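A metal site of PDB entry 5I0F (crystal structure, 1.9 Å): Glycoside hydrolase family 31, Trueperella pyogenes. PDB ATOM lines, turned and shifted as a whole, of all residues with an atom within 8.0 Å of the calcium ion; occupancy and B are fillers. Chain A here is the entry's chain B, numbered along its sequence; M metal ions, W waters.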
ATOM      1  N   ARG A   7      -8.401  22.325 -25.766  1.00  0.00           N
ATOM      2  CA  ARG A   7      -9.594  21.450 -25.693  1.00  0.00           C
ATOM      3  C   ARG A   7      -9.440  20.143 -26.445  1.00  0.00           C
ATOM      4  O   ARG A   7     -10.335  19.287 -26.381  1.00  0.00           O
ATOM      5  CB  ARG A   7     -10.828  22.202 -26.186  1.00  0.00           C
ATOM      6  CG  ARG A   7     -11.288  23.311 -25.250  1.00  0.00           C
ATOM      7  CD  ARG A   7     -12.418  24.128 -25.891  1.00  0.00           C
ATOM      8  NE  ARG A   7     -11.839  25.291 -26.541  1.00  0.00           N
ATOM      9  CZ  ARG A   7     -11.631  25.467 -27.843  1.00  0.00           C
ATOM     10  NH1 ARG A   7     -11.991  24.576 -28.742  1.00  0.00           N
ATOM     11  NH2 ARG A   7     -11.061  26.592 -28.249  1.00  0.00           N
ATOM     12  N   ILE A  24     -11.223  22.987 -19.121  1.00  0.00           N
ATOM     13  CA  ILE A  24     -11.407  24.265 -18.395  1.00  0.00           C
ATOM     14  C   ILE A  24     -10.757  24.062 -17.014  1.00  0.00           C
ATOM     15  O   ILE A  24     -11.350  23.420 -16.130  1.00  0.00           O
ATOM     16  CB  ILE A  24     -12.920  24.619 -18.221  1.00  0.00           C
ATOM     17  CG1 ILE A  24     -13.614  24.752 -19.596  1.00  0.00           C
ATOM     18  CG2 ILE A  24     -13.109  25.871 -17.363  1.00  0.00           C
ATOM     19  CD1 ILE A  24     -13.064  25.849 -20.491  1.00  0.00           C
ATOM     20  N   THR A 160     -17.631  33.308 -17.446  1.00  0.00           N
ATOM     21  CA  THR A 160     -18.437  32.305 -16.741  1.00  0.00           C
ATOM     22  C   THR A 160     -18.680  31.124 -17.673  1.00  0.00           C
ATOM     23  O   THR A 160     -19.259  31.296 -18.754  1.00  0.00           O
ATOM     24  CB  THR A 160     -19.780  32.930 -16.280  1.00  0.00           C
ATOM     25  OG1 THR A 160     -19.500  34.136 -15.581  1.00  0.00           O
ATOM     26  CG2 THR A 160     -20.544  31.991 -15.360  1.00  0.00           C
ATOM     27  N   HIS A 161     -18.225  29.947 -17.280  1.00  0.00           N
ATOM     28  CA  HIS A 161     -18.120  28.820 -18.215  1.00  0.00           C
ATOM     29  C   HIS A 161     -19.224  27.783 -18.092  1.00  0.00           C
ATOM     30  O   HIS A 161     -19.641  27.204 -19.103  1.00  0.00           O
ATOM     31  CB  HIS A 161     -16.764  28.139 -18.071  1.00  0.00           C
ATOM     32  CG  HIS A 161     -15.625  29.102 -18.120  1.00  0.00           C
ATOM     33  ND1 HIS A 161     -15.182  29.672 -19.285  1.00  0.00           N
ATOM     34  CD2 HIS A 161     -14.863  29.634 -17.135  1.00  0.00           C
ATOM     35  CE1 HIS A 161     -14.188  30.498 -19.030  1.00  0.00           C
ATOM     36  NE2 HIS A 161     -13.973  30.502 -17.722  1.00  0.00           N
ATOM     37  N   ARG A 162     -19.648  27.523 -16.859  1.00  0.00           N
ATOM     38  CA  ARG A 162     -20.684  26.518 -16.549  1.00  0.00           C
ATOM     39  C   ARG A 162     -21.504  26.969 -15.347  1.00  0.00           C
ATOM     40  O   ARG A 162     -21.084  27.843 -14.578  1.00  0.00           O
ATOM     41  CB  ARG A 162     -20.068  25.146 -16.246  1.00  0.00           C
ATOM     42  CG  ARG A 162     -19.352  24.501 -17.432  1.00  0.00           C
ATOM     43  CD  ARG A 162     -19.390  22.980 -17.393  1.00  0.00           C
ATOM     44  NE  ARG A 162     -18.650  22.466 -16.252  1.00  0.00           N
ATOM     45  CZ  ARG A 162     -17.323  22.304 -16.205  1.00  0.00           C
ATOM     46  NH1 ARG A 162     -16.545  22.632 -17.232  1.00  0.00           N
ATOM     47  NH2 ARG A 162     -16.767  21.821 -15.112  1.00  0.00           N
ATOM     48  N   ARG A 234     -26.593  23.626 -25.856  1.00  0.00           N
ATOM     49  CA  ARG A 234     -25.288  23.287 -25.314  1.00  0.00           C
ATOM     50  C   ARG A 234     -25.420  22.017 -24.488  1.00  0.00           C
ATOM     51  O   ARG A 234     -26.509  21.568 -24.166  1.00  0.00           O
ATOM     52  CB  ARG A 234     -24.716  24.432 -24.458  1.00  0.00           C
ATOM     53  CG  ARG A 234     -24.616  25.743 -25.207  1.00  0.00           C
ATOM     54  CD  ARG A 234     -23.697  26.753 -24.511  1.00  0.00           C
ATOM     55  NE  ARG A 234     -23.598  28.025 -25.226  1.00  0.00           N
ATOM     56  CZ  ARG A 234     -24.456  29.047 -25.156  1.00  0.00           C
ATOM     57  NH1 ARG A 234     -25.572  28.992 -24.411  1.00  0.00           N
ATOM     58  NH2 ARG A 234     -24.220  30.160 -25.864  1.00  0.00           N
ATOM     59  N   ARG A 235     -24.270  21.440 -24.155  1.00  0.00           N
ATOM     60  CA  ARG A 235     -24.226  20.195 -23.405  1.00  0.00           C
ATOM     61  C   ARG A 235     -24.738  20.412 -21.984  1.00  0.00           C
ATOM     62  O   ARG A 235     -24.514  21.477 -21.394  1.00  0.00           O
ATOM     63  CB  ARG A 235     -22.805  19.681 -23.376  1.00  0.00           C
ATOM     64  CG  ARG A 235     -22.642  18.308 -22.780  1.00  0.00           C
ATOM     65  CD  ARG A 235     -21.272  17.796 -23.130  1.00  0.00           C
ATOM     66  NE  ARG A 235     -21.027  16.424 -22.687  1.00  0.00           N
ATOM     67  CZ  ARG A 235     -19.855  15.803 -22.864  1.00  0.00           C
ATOM     68  NH1 ARG A 235     -19.692  14.558 -22.458  1.00  0.00           N
ATOM     69  NH2 ARG A 235     -18.829  16.456 -23.419  1.00  0.00           N
ATOM     70  N   VAL A 252     -24.778  22.810 -16.698  1.00  0.00           N
ATOM     71  CA  VAL A 252     -25.069  23.356 -18.003  1.00  0.00           C
ATOM     72  C   VAL A 252     -23.827  24.077 -18.519  1.00  0.00           C
ATOM     73  O   VAL A 252     -23.246  24.934 -17.813  1.00  0.00           O
ATOM     74  CB  VAL A 252     -26.238  24.362 -17.895  1.00  0.00           C
ATOM     75  CG1 VAL A 252     -26.600  24.920 -19.249  1.00  0.00           C
ATOM     76  CG2 VAL A 252     -27.444  23.737 -17.207  1.00  0.00           C
ATOM     77  N   ASP A 253     -23.407  23.729 -19.728  1.00  0.00           N
ATOM     78  CA  ASP A 253     -22.353  24.499 -20.423  1.00  0.00           C
ATOM     79  C   ASP A 253     -22.915  25.862 -20.827  1.00  0.00           C
ATOM     80  O   ASP A 253     -24.069  25.962 -21.275  1.00  0.00           O
ATOM     81  CB  ASP A 253     -21.832  23.722 -21.634  1.00  0.00           C
ATOM     82  CG  ASP A 253     -20.838  24.499 -22.458  1.00  0.00           C
ATOM     83  OD1 ASP A 253     -19.907  25.103 -21.884  1.00  0.00           O
ATOM     84  OD2 ASP A 253     -20.973  24.533 -23.711  1.00  0.00           O
ATOM     85  N   LEU A 254     -22.114  26.915 -20.652  1.00  0.00           N
ATOM     86  CA  LEU A 254     -22.492  28.276 -21.021  1.00  0.00           C
ATOM     87  C   LEU A 254     -21.713  28.775 -22.240  1.00  0.00           C
ATOM     88  O   LEU A 254     -20.899  28.046 -22.771  1.00  0.00           O
ATOM     89  CB  LEU A 254     -22.293  29.207 -19.829  1.00  0.00           C
ATOM     90  CG  LEU A 254     -23.166  28.868 -18.598  1.00  0.00           C
ATOM     91  CD1 LEU A 254     -22.792  29.770 -17.439  1.00  0.00           C
ATOM     92  CD2 LEU A 254     -24.642  28.972 -18.928  1.00  0.00           C
ATOM     93  N   GLY A 255     -21.990  30.005 -22.692  1.00  0.00           N
ATOM     94  CA  GLY A 255     -21.364  30.609 -23.905  1.00  0.00           C
ATOM     95  C   GLY A 255     -19.845  30.789 -23.937  1.00  0.00           C
ATOM     96  O   GLY A 255     -19.119  30.263 -23.086  1.00  0.00           O
ATOM     97  N   PHE A 256     -19.358  31.518 -24.945  1.00  0.00           N
ATOM     98  CA  PHE A 256     -17.902  31.671 -25.194  1.00  0.00           C
ATOM     99  C   PHE A 256     -17.471  33.130 -25.039  1.00  0.00           C
ATOM    100  O   PHE A 256     -17.788  33.773 -24.034  1.00  0.00           O
ATOM    101  CB  PHE A 256     -17.561  31.182 -26.613  1.00  0.00           C
ATOM    102  CG  PHE A 256     -16.242  30.427 -26.713  1.00  0.00           C
ATOM    103  CD1 PHE A 256     -15.081  30.880 -26.074  1.00  0.00           C
ATOM    104  CD2 PHE A 256     -16.170  29.262 -27.494  1.00  0.00           C
ATOM    105  CE1 PHE A 256     -13.881  30.177 -26.195  1.00  0.00           C
ATOM    106  CE2 PHE A 256     -14.963  28.566 -27.616  1.00  0.00           C
ATOM    107  CZ  PHE A 256     -13.829  29.020 -26.966  1.00  0.00           C
ATOM    108  N   SER A 475     -16.028  23.297 -29.899  1.00  0.00           N
ATOM    109  CA  SER A 475     -16.867  24.309 -29.288  1.00  0.00           C
ATOM    110  C   SER A 475     -16.823  25.650 -30.047  1.00  0.00           C
ATOM    111  O   SER A 475     -17.759  26.436 -29.948  1.00  0.00           O
ATOM    112  CB  SER A 475     -16.450  24.523 -27.820  1.00  0.00           C
ATOM    113  OG  SER A 475     -15.190  25.192 -27.780  1.00  0.00           O
ATOM    114  N   ASP A 476     -15.751  25.882 -30.813  1.00  0.00           N
ATOM    115  CA  ASP A 476     -15.495  27.166 -31.494  1.00  0.00           C
ATOM    116  C   ASP A 476     -15.730  27.120 -33.009  1.00  0.00           C
ATOM    117  O   ASP A 476     -15.385  28.074 -33.708  1.00  0.00           O
ATOM    118  CB  ASP A 476     -14.098  27.702 -31.177  1.00  0.00           C
ATOM    119  CG  ASP A 476     -13.007  26.623 -31.239  1.00  0.00           C
ATOM    120  OD1 ASP A 476     -13.284  25.401 -31.485  1.00  0.00           O
ATOM    121  OD2 ASP A 476     -11.835  27.013 -30.967  1.00  0.00           O
ATOM    122  N   ARG A 484     -21.898  29.318 -32.453  1.00  0.00           N
ATOM    123  CA  ARG A 484     -20.638  28.596 -32.415  1.00  0.00           C
ATOM    124  C   ARG A 484     -20.962  27.131 -32.211  1.00  0.00           C
ATOM    125  O   ARG A 484     -22.120  26.764 -31.964  1.00  0.00           O
ATOM    126  CB  ARG A 484     -19.719  29.104 -31.302  1.00  0.00           C
ATOM    127  CG  ARG A 484     -19.384  30.587 -31.356  1.00  0.00           C
ATOM    128  CD  ARG A 484     -18.956  31.079 -32.717  1.00  0.00           C
ATOM    129  NE  ARG A 484     -17.605  30.672 -33.094  1.00  0.00           N
ATOM    130  CZ  ARG A 484     -16.473  31.263 -32.704  1.00  0.00           C
ATOM    131  NH1 ARG A 484     -15.295  30.800 -33.143  1.00  0.00           N
ATOM    132  NH2 ARG A 484     -16.485  32.310 -31.866  1.00  0.00           N
ATOM    133  N   GLY A 485     -19.949  26.294 -32.288  1.00  0.00           N
ATOM    134  CA  GLY A 485     -20.168  24.853 -32.209  1.00  0.00           C
ATOM    135  C   GLY A 485     -20.760  24.382 -30.906  1.00  0.00           C
ATOM    136  O   GLY A 485     -21.539  23.413 -30.887  1.00  0.00           O
ATOM    137  N   ASP A 486     -20.416  25.047 -29.820  1.00  0.00           N
ATOM    138  CA  ASP A 486     -20.978  24.660 -28.534  1.00  0.00           C
ATOM    139  C   ASP A 486     -22.504  24.708 -28.477  1.00  0.00           C
ATOM    140  O   ASP A 486     -23.087  23.974 -27.677  1.00  0.00           O
ATOM    141  CB  ASP A 486     -20.346  25.447 -27.393  1.00  0.00           C
ATOM    142  CG  ASP A 486     -20.726  26.906 -27.387  1.00  0.00           C
ATOM    143  OD1 ASP A 486     -20.981  27.495 -28.466  1.00  0.00           O
ATOM    144  OD2 ASP A 486     -20.725  27.468 -26.284  1.00  0.00           O
ATOM    145  N   GLU A 487     -23.129  25.508 -29.340  1.00  0.00           N
ATOM    146  CA  GLU A 487     -24.594  25.463 -29.560  1.00  0.00           C
ATOM    147  C   GLU A 487     -25.021  24.739 -30.821  1.00  0.00           C
ATOM    148  O   GLU A 487     -26.033  24.072 -30.837  1.00  0.00           O
ATOM    149  CB  GLU A 487     -25.161  26.892 -29.647  1.00  0.00           C
ATOM    150  CG  GLU A 487     -25.213  27.632 -28.355  1.00  0.00           C
ATOM    151  CD  GLU A 487     -26.004  28.944 -28.478  1.00  0.00           C
ATOM    152  OE1 GLU A 487     -25.524  29.875 -29.149  1.00  0.00           O
ATOM    153  OE2 GLU A 487     -27.113  29.024 -27.914  1.00  0.00           O
HETATM  154 CA    CA M   1     -19.483  26.673 -23.933  1.00  0.00          CA
HETATM  155  O   HOH W   1     -18.043  24.947 -24.559  1.00  0.00           O
HETATM  156  O   HOH W   2     -18.123  28.340 -25.151  1.00  0.00           O
HETATM  157  O   HOH W   3     -18.324  27.521 -21.838  1.00  0.00           O
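Merely in contact with the calcium ion: Gly 255 (3.7 Å).
Of the 18 residues printed, 4 come within 4 Å of the calcium ion.
The nearest printed residue that does not touch the calcium ion is Arg 234 (4.3 Å).
The backbone NH (N) of Asp 253 is in hydrogen-bond range of the backbone carbonyl oxygen (O) of Arg 235.
The guanidinium group of Arg 234 lies close to the side-chain carboxylate of Asp 486 (3.1 Å).
O of His 161 is in hydrogen-bond range of N of Leu 254 (2.9 Å).
The backbone carbonyl oxygen (O) of Ser 475 lies within hydrogen-bond range of the backbone NH (N) of Asp 486 (3.0 Å).
Water W3 lies within hydrogen-bond range of O of His 161 and O of Gly 255.
The calcium ion is bound by the backbone carbonyl oxygen (O) of Leu 254, water W1, water W2, water W3, the side-chain carboxylate (OD1) of Asp 253, the side-chain carboxylate (OD2) of Asp 253 and the side-chain carboxylate (OD2) of Asp 486.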
